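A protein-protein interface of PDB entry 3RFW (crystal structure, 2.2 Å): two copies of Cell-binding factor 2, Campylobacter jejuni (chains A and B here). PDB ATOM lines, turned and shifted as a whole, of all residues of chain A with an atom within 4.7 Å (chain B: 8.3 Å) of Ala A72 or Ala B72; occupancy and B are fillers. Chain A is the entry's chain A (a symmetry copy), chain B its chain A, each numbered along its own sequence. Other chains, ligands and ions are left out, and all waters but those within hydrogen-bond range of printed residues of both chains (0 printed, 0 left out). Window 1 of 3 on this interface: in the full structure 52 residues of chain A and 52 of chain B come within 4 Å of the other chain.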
ATOM      1  N   GLU A  68       0.785   1.807 -18.825  1.00  0.00           N
ATOM      2  CA  GLU A  68       1.745   1.945 -17.737  1.00  0.00           C
ATOM      3  C   GLU A  68       1.093   1.810 -16.388  1.00  0.00           C
ATOM      4  O   GLU A  68       1.688   1.300 -15.462  1.00  0.00           O
ATOM      5  CB  GLU A  68       2.551   3.238 -17.846  1.00  0.00           C
ATOM      6  CG  GLU A  68       3.483   3.242 -19.079  1.00  0.00           C
ATOM      7  CD  GLU A  68       4.422   2.027 -19.134  1.00  0.00           C
ATOM      8  OE1 GLU A  68       5.145   1.784 -18.130  1.00  0.00           O
ATOM      9  OE2 GLU A  68       4.462   1.346 -20.198  1.00  0.00           O
ATOM     10  N   LEU A  69      -0.159   2.215 -16.293  1.00  0.00           N
ATOM     11  CA  LEU A  69      -0.907   1.990 -15.090  1.00  0.00           C
ATOM     12  C   LEU A  69      -1.154   0.489 -14.859  1.00  0.00           C
ATOM     13  O   LEU A  69      -1.076   0.045 -13.710  1.00  0.00           O
ATOM     14  CB  LEU A  69      -2.236   2.737 -15.107  1.00  0.00           C
ATOM     15  CG  LEU A  69      -3.142   2.501 -13.907  1.00  0.00           C
ATOM     16  CD1 LEU A  69      -2.463   2.948 -12.646  1.00  0.00           C
ATOM     17  CD2 LEU A  69      -4.528   3.129 -14.094  1.00  0.00           C
ATOM     18  N   ASP A  70      -1.466  -0.272 -15.920  1.00  0.00           N
ATOM     19  CA  ASP A  70      -1.618  -1.740 -15.770  1.00  0.00           C
ATOM     20  C   ASP A  70      -0.317  -2.325 -15.251  1.00  0.00           C
ATOM     21  O   ASP A  70      -0.340  -3.151 -14.355  1.00  0.00           O
ATOM     22  CB  ASP A  70      -1.995  -2.448 -17.081  1.00  0.00           C
ATOM     23  CG  ASP A  70      -3.456  -2.258 -17.455  1.00  0.00           C
ATOM     24  OD1 ASP A  70      -4.274  -1.913 -16.562  1.00  0.00           O
ATOM     25  OD2 ASP A  70      -3.769  -2.354 -18.665  1.00  0.00           O
ATOM     26  N   ARG A  71       0.810  -1.876 -15.803  1.00  0.00           N
ATOM     27  CA  ARG A  71       2.110  -2.365 -15.396  1.00  0.00           C
ATOM     28  C   ARG A  71       2.390  -2.026 -13.930  1.00  0.00           C
ATOM     29  O   ARG A  71       2.812  -2.888 -13.171  1.00  0.00           O
ATOM     30  CB  ARG A  71       3.203  -1.779 -16.304  1.00  0.00           C
ATOM     31  CG  ARG A  71       4.578  -2.416 -16.124  1.00  0.00           C
ATOM     32  CD  ARG A  71       5.705  -1.696 -16.901  1.00  0.00           C
ATOM     33  NE  ARG A  71       5.304  -1.303 -18.255  1.00  0.00           N
ATOM     34  CZ  ARG A  71       5.360  -2.071 -19.349  1.00  0.00           C
ATOM     35  NH1 ARG A  71       5.782  -3.327 -19.292  1.00  0.00           N
ATOM     36  NH2 ARG A  71       4.944  -1.579 -20.515  1.00  0.00           N
ATOM     37  N   ALA A  72       2.164  -0.767 -13.535  1.00  0.00           N
ATOM     38  CA  ALA A  72       2.424  -0.323 -12.159  1.00  0.00           C
ATOM     39  C   ALA A  72       1.552  -1.102 -11.183  1.00  0.00           C
ATOM     40  O   ALA A  72       1.970  -1.466 -10.083  1.00  0.00           O
ATOM     41  CB  ALA A  72       2.137   1.257 -12.009  1.00  0.00           C
ATOM     42  N   LYS A  73       0.302  -1.285 -11.538  1.00  0.00           N
ATOM     43  CA  LYS A  73      -0.618  -1.981 -10.641  1.00  0.00           C
ATOM     44  C   LYS A  73      -0.122  -3.438 -10.316  1.00  0.00           C
ATOM     45  O   LYS A  73       0.013  -3.807  -9.142  1.00  0.00           O
ATOM     46  CB  LYS A  73      -1.995  -1.939 -11.308  1.00  0.00           C
ATOM     47  CG  LYS A  73      -3.049  -2.911 -10.836  1.00  0.00           C
ATOM     48  CD  LYS A  73      -4.427  -2.267 -11.026  1.00  0.00           C
ATOM     49  CE  LYS A  73      -5.375  -3.149 -11.833  1.00  0.00           C
ATOM     50  NZ  LYS A  73      -4.941  -3.228 -13.260  1.00  0.00           N
ATOM     51  N   ASP A  74       0.302  -4.179 -11.351  1.00  0.00           N
ATOM     52  CA  ASP A  74       0.903  -5.507 -11.181  1.00  0.00           C
ATOM     53  C   ASP A  74       2.239  -5.447 -10.433  1.00  0.00           C
ATOM     54  O   ASP A  74       2.428  -6.159  -9.442  1.00  0.00           O
ATOM     55  CB  ASP A  74       1.016  -6.268 -12.554  1.00  0.00           C
ATOM     56  CG  ASP A  74      -0.351  -6.714 -13.079  1.00  0.00           C
ATOM     57  OD1 ASP A  74      -1.341  -6.570 -12.335  1.00  0.00           O
ATOM     58  OD2 ASP A  74      -0.478  -7.204 -14.225  1.00  0.00           O
ATOM     59  N   ALA A  75       3.096  -4.488 -10.771  1.00  0.00           N
ATOM     60  CA  ALA A  75       4.400  -4.449 -10.125  1.00  0.00           C
ATOM     61  C   ALA A  75       4.313  -4.059  -8.662  1.00  0.00           C
ATOM     62  O   ALA A  75       5.091  -4.523  -7.846  1.00  0.00           O
ATOM     63  CB  ALA A  75       5.367  -3.503 -10.878  1.00  0.00           C
ATOM     64  N   ILE A  76       3.360  -3.199  -8.316  1.00  0.00           N
ATOM     65  CA  ILE A  76       3.224  -2.816  -6.922  1.00  0.00           C
ATOM     66  C   ILE A  76       2.664  -3.966  -6.092  1.00  0.00           C
ATOM     67  O   ILE A  76       3.088  -4.180  -4.969  1.00  0.00           O
ATOM     68  CB  ILE A  76       2.316  -1.575  -6.732  1.00  0.00           C
ATOM     69  CG1 ILE A  76       2.957  -0.332  -7.364  1.00  0.00           C
ATOM     70  CG2 ILE A  76       1.990  -1.423  -5.272  1.00  0.00           C
ATOM     71  CD1 ILE A  76       1.921   0.854  -7.681  1.00  0.00           C
ATOM     72  N   LEU B  51       0.786 -12.903  -8.451  1.00  0.00           N
ATOM     73  CA  LEU B  51      -0.386 -11.977  -8.482  1.00  0.00           C
ATOM     74  C   LEU B  51      -1.662 -12.659  -7.976  1.00  0.00           C
ATOM     75  O   LEU B  51      -2.368 -12.117  -7.141  1.00  0.00           O
ATOM     76  CB  LEU B  51      -0.631 -11.456  -9.916  1.00  0.00           C
ATOM     77  CG  LEU B  51       0.342 -10.402 -10.484  1.00  0.00           C
ATOM     78  CD1 LEU B  51       0.046 -10.132 -11.953  1.00  0.00           C
ATOM     79  CD2 LEU B  51       0.352  -9.057  -9.686  1.00  0.00           C
ATOM     80  N   TYR B  65      -0.511  -1.166  -0.740  1.00  0.00           N
ATOM     81  CA  TYR B  65      -0.859  -1.237  -2.153  1.00  0.00           C
ATOM     82  C   TYR B  65      -1.648   0.003  -2.608  1.00  0.00           C
ATOM     83  O   TYR B  65      -1.300   0.634  -3.601  1.00  0.00           O
ATOM     84  CB  TYR B  65      -1.635  -2.508  -2.442  1.00  0.00           C
ATOM     85  CG  TYR B  65      -2.162  -2.595  -3.855  1.00  0.00           C
ATOM     86  CD1 TYR B  65      -1.336  -3.005  -4.897  1.00  0.00           C
ATOM     87  CD2 TYR B  65      -3.486  -2.255  -4.148  1.00  0.00           C
ATOM     88  CE1 TYR B  65      -1.815  -3.061  -6.214  1.00  0.00           C
ATOM     89  CE2 TYR B  65      -3.966  -2.312  -5.443  1.00  0.00           C
ATOM     90  CZ  TYR B  65      -3.119  -2.731  -6.461  1.00  0.00           C
ATOM     91  OH  TYR B  65      -3.575  -2.797  -7.748  1.00  0.00           O
ATOM     92  N   THR B  66      -2.718   0.348  -1.895  1.00  0.00           N
ATOM     93  CA  THR B  66      -3.674   1.327  -2.437  1.00  0.00           C
ATOM     94  C   THR B  66      -3.058   2.723  -2.468  1.00  0.00           C
ATOM     95  O   THR B  66      -3.245   3.485  -3.415  1.00  0.00           O
ATOM     96  CB  THR B  66      -4.953   1.419  -1.597  1.00  0.00           C
ATOM     97  OG1 THR B  66      -4.601   1.669  -0.244  1.00  0.00           O
ATOM     98  CG2 THR B  66      -5.809   0.176  -1.706  1.00  0.00           C
ATOM     99  N   LYS B  67      -2.274   3.029  -1.452  1.00  0.00           N
ATOM    100  CA  LYS B  67      -1.590   4.295  -1.357  1.00  0.00           C
ATOM    101  C   LYS B  67      -0.487   4.440  -2.419  1.00  0.00           C
ATOM    102  O   LYS B  67      -0.281   5.535  -2.954  1.00  0.00           O
ATOM    103  CB  LYS B  67      -1.010   4.433   0.043  1.00  0.00           C
ATOM    104  CG  LYS B  67      -0.368   5.761   0.353  1.00  0.00           C
ATOM    105  CD  LYS B  67      -0.281   5.925   1.871  1.00  0.00           C
ATOM    106  CE  LYS B  67       1.044   6.553   2.289  1.00  0.00           C
ATOM    107  NZ  LYS B  67       2.203   5.639   2.071  1.00  0.00           N
ATOM    108  N   GLU B  68       0.200   3.352  -2.766  1.00  0.00           N
ATOM    109  CA  GLU B  68       1.215   3.463  -3.805  1.00  0.00           C
ATOM    110  C   GLU B  68       0.616   3.440  -5.185  1.00  0.00           C
ATOM    111  O   GLU B  68       1.110   4.087  -6.085  1.00  0.00           O
ATOM    112  CB  GLU B  68       2.310   2.408  -3.651  1.00  0.00           C
ATOM    113  CG  GLU B  68       3.154   2.627  -2.374  1.00  0.00           C
ATOM    114  CD  GLU B  68       3.760   4.037  -2.282  1.00  0.00           C
ATOM    115  OE1 GLU B  68       4.447   4.457  -3.252  1.00  0.00           O
ATOM    116  OE2 GLU B  68       3.579   4.699  -1.221  1.00  0.00           O
ATOM    117  N   LEU B  69      -0.491   2.739  -5.338  1.00  0.00           N
ATOM    118  CA  LEU B  69      -1.213   2.779  -6.577  1.00  0.00           C
ATOM    119  C   LEU B  69      -1.813   4.173  -6.828  1.00  0.00           C
ATOM    120  O   LEU B  69      -1.792   4.630  -7.975  1.00  0.00           O
ATOM    121  CB  LEU B  69      -2.316   1.726  -6.618  1.00  0.00           C
ATOM    122  CG  LEU B  69      -3.193   1.738  -7.862  1.00  0.00           C
ATOM    123  CD1 LEU B  69      -2.365   1.481  -9.086  1.00  0.00           C
ATOM    124  CD2 LEU B  69      -4.388   0.786  -7.737  1.00  0.00           C
ATOM    125  N   ASP B  70      -2.354   4.827  -5.788  1.00  0.00           N
ATOM    126  CA  ASP B  70      -2.856   6.213  -5.954  1.00  0.00           C
ATOM    127  C   ASP B  70      -1.717   7.104  -6.413  1.00  0.00           C
ATOM    128  O   ASP B  70      -1.901   7.905  -7.314  1.00  0.00           O
ATOM    129  CB  ASP B  70      -3.459   6.797  -4.666  1.00  0.00           C
ATOM    130  CG  ASP B  70      -4.844   6.251  -4.362  1.00  0.00           C
ATOM    131  OD1 ASP B  70      -5.507   5.720  -5.291  1.00  0.00           O
ATOM    132  OD2 ASP B  70      -5.229   6.259  -3.169  1.00  0.00           O
ATOM    133  N   ARG B  71      -0.542   6.945  -5.806  1.00  0.00           N
ATOM    134  CA  ARG B  71       0.615   7.743  -6.152  1.00  0.00           C
ATOM    135  C   ARG B  71       1.040   7.493  -7.602  1.00  0.00           C
ATOM    136  O   ARG B  71       1.272   8.437  -8.345  1.00  0.00           O
ATOM    137  CB  ARG B  71       1.775   7.440  -5.190  1.00  0.00           C
ATOM    138  CG  ARG B  71       2.956   8.398  -5.308  1.00  0.00           C
ATOM    139  CD  ARG B  71       4.187   7.974  -4.473  1.00  0.00           C
ATOM    140  NE  ARG B  71       3.832   7.486  -3.137  1.00  0.00           N
ATOM    141  CZ  ARG B  71       3.643   8.237  -2.046  1.00  0.00           C
ATOM    142  NH1 ARG B  71       3.745   9.559  -2.091  1.00  0.00           N
ATOM    143  NH2 ARG B  71       3.307   7.651  -0.899  1.00  0.00           N
ATOM    144  N   ALA B  72       1.152   6.219  -7.999  1.00  0.00           N
ATOM    145  CA  ALA B  72       1.578   5.861  -9.358  1.00  0.00           C
ATOM    146  C   ALA B  72       0.589   6.407 -10.379  1.00  0.00           C
ATOM    147  O   ALA B  72       0.957   6.869 -11.460  1.00  0.00           O
ATOM    148  CB  ALA B  72       1.699   4.260  -9.513  1.00  0.00           C
ATOM    149  N   LYS B  73      -0.683   6.273 -10.086  1.00  0.00           N
ATOM    150  CA  LYS B  73      -1.702   6.725 -11.030  1.00  0.00           C
ATOM    151  C   LYS B  73      -1.567   8.261 -11.340  1.00  0.00           C
ATOM    152  O   LYS B  73      -1.472   8.659 -12.509  1.00  0.00           O
ATOM    153  CB  LYS B  73      -3.057   6.339 -10.430  1.00  0.00           C
ATOM    154  CG  LYS B  73      -4.294   7.024 -10.958  1.00  0.00           C
ATOM    155  CD  LYS B  73      -5.478   6.057 -10.830  1.00  0.00           C
ATOM    156  CE  LYS B  73      -6.652   6.673 -10.075  1.00  0.00           C
ATOM    157  NZ  LYS B  73      -6.320   6.849  -8.629  1.00  0.00           N
ATOM    158  N   ASP B  74      -1.390   9.078 -10.290  1.00  0.00           N
ATOM    159  CA  ASP B  74      -1.128  10.514 -10.439  1.00  0.00           C
ATOM    160  C   ASP B  74       0.216  10.790 -11.122  1.00  0.00           C
ATOM    161  O   ASP B  74       0.270  11.533 -12.108  1.00  0.00           O
ATOM    162  CB  ASP B  74      -1.273  11.271  -9.067  1.00  0.00           C
ATOM    163  CG  ASP B  74      -2.731  11.362  -8.611  1.00  0.00           C
ATOM    164  OD1 ASP B  74      -3.618  10.982  -9.400  1.00  0.00           O
ATOM    165  OD2 ASP B  74      -3.030  11.798  -7.476  1.00  0.00           O
ATOM    166  N   ALA B  75       1.266  10.071 -10.737  1.00  0.00           N
ATOM    167  CA  ALA B  75       2.568  10.360 -11.320  1.00  0.00           C
ATOM    168  C   ALA B  75       2.651   9.970 -12.783  1.00  0.00           C
ATOM    169  O   ALA B  75       3.328  10.616 -13.564  1.00  0.00           O
ATOM    170  CB  ALA B  75       3.702   9.677 -10.516  1.00  0.00           C
ATOM    171  N   ILE B  76       1.957   8.903 -13.170  1.00  0.00           N
ATOM    172  CA  ILE B  76       1.988   8.507 -14.566  1.00  0.00           C
ATOM    173  C   ILE B  76       1.201   9.487 -15.429  1.00  0.00           C
ATOM    174  O   ILE B  76       1.612   9.806 -16.531  1.00  0.00           O
ATOM    175  CB  ILE B  76       1.424   7.080 -14.792  1.00  0.00           C
ATOM    176  CG1 ILE B  76       2.322   6.031 -14.122  1.00  0.00           C
ATOM    177  CG2 ILE B  76       1.217   6.861 -16.265  1.00  0.00           C
ATOM    178  CD1 ILE B  76       1.597   4.623 -13.848  1.00  0.00           C
ATOM    179  N   LEU B  77       0.052   9.941 -14.954  1.00  0.00           N
ATOM    180  CA  LEU B  77      -0.729  10.952 -15.717  1.00  0.00           C
ATOM    181  C   LEU B  77       0.077  12.273 -15.931  1.00  0.00           C
ATOM    182  O   LEU B  77       0.045  12.870 -17.013  1.00  0.00           O
ATOM    183  CB  LEU B  77      -2.036  11.283 -14.980  1.00  0.00           C
ATOM    184  CG  LEU B  77      -3.074  12.075 -15.793  1.00  0.00           C
ATOM    185  CD1 LEU B  77      -3.369  11.373 -17.120  1.00  0.00           C
ATOM    186  CD2 LEU B  77      -4.374  12.345 -15.010  1.00  0.00           C
ATOM    187  N   VAL B  78       0.761  12.739 -14.885  1.00  0.00           N
ATOM    188  CA  VAL B  78       1.561  13.953 -14.961  1.00  0.00           C
ATOM    189  C   VAL B  78       2.667  13.755 -15.991  1.00  0.00           C
ATOM    190  O   VAL B  78       2.928  14.627 -16.800  1.00  0.00           O
ATOM    191  CB  VAL B  78       2.143  14.329 -13.596  1.00  0.00           C
ATOM    192  CG1 VAL B  78       3.281  15.380 -13.740  1.00  0.00           C
ATOM    193  CG2 VAL B  78       1.071  14.853 -12.697  1.00  0.00           C
ATOM    194  N   ASN B  79       3.234  12.556 -16.036  1.00  0.00           N
ATOM    195  CA  ASN B  79       4.319  12.266 -16.955  1.00  0.00           C
ATOM    196  C   ASN B  79       3.829  12.187 -18.388  1.00  0.00           C
ATOM    197  O   ASN B  79       4.493  12.653 -19.305  1.00  0.00           O
ATOM    198  CB  ASN B  79       4.978  10.953 -16.563  1.00  0.00           C
ATOM    199  CG  ASN B  79       6.230  10.682 -17.349  1.00  0.00           C
ATOM    200  OD1 ASN B  79       6.199   9.973 -18.351  1.00  0.00           O
ATOM    201  ND2 ASN B  79       7.332  11.307 -16.945  1.00  0.00           N
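The side-chain carboxylate of Glu A68 lies within salt-bridge range of the guanidinium group of Arg A71 (3.0 Å). The side-chain amino group (NZ) of Lys B67 is in salt-bridge range of the side-chain carboxylate (OE2) of Glu B68 (3.7 Å). OD1 of Asp A70 lies within salt-bridge range of NZ of Lys A73, at 3.6 Å. OE2 of Glu B68 lies within salt-bridge range of NH2 of Arg B71 (3.0 Å).
Ile B76 touches Glu A68. Leu A69 touches Leu B69. Leu A69 touches Ile B76 (CA to CD1, 3.8 Å). CB of Ala A72 touches CB of Ala B72, at 3.9 Å. CG of Lys A73 touches OH of Tyr B65, 3.1 Å away. Asp A74 touches Leu B51 (O to CD2, 3.6 Å). Tyr B65 touches Ile A76 (CD1 to CG2, 3.7 Å). Glu B68 touches Ile A76. Leu B69 touches Ile A76 (CA to CD1, 3.8 Å). Ala B72 touches Ile A76.
Of chain B, only Ala B72 and Ile B76 come within 4 Å of Ala A72. Ala B72 touches two residues of chain A. Of the printed residues of chain A, Ile B76 touches Glu A68 (3.7 Å), Leu A69 (3.8 Å) and Ala A72 (3.9 Å). Of the printed residues of chain B, Leu A69 touches Leu B69 and Ile B76. Of the printed residues of chain B, Asp A74 touches Leu B51. Of the printed residues of chain A, Leu B51 touches Asp A74 (3.6 Å). Asp B74 touches none of the printed residues of chain A. The nearest residue of chain B that does not touch Ala A72 is Leu B69 (5.1 Å). The nearest printed residue of chain B that does not touch Ile A76 is Thr B66 (6.1 Å).
Hydrophobic or aromatic side chains of chain B that line the printed part of chain A: Leu B51, Tyr B65, Leu B69, Ala B72 and Ile B76. Of the 9 printed residues of chain A, 6 touch a printed residue of chain B. Printed residues of chain A that touch a printed residue of chain B: Glu A68, Leu A69, Ala A72, Lys A73, Asp A74 and Ile A76. Among the printed residues, 11 pairs touch across the chains. Among the printed residues, no Asp or Glu carboxylate lies within 4 Å of a Lys or Arg side-chain nitrogen of the other chain.
Glu A68 touches Ile B76, and with the chains exchanged Ile A76 touches Glu B68. Leu A69 touches Ile B76, and with the chains exchanged Ile A76 touches Leu B69. Ala A72 touches its own counterpart, Ala B72. Ala A72 touches Ile B76, and with the chains exchanged Ile A76 touches Ala B72. 9 positions are printed for both chains. Of the 11 pairs that touch across the chains among the printed residues, 8 have their exchanged pair printed and touching as well.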
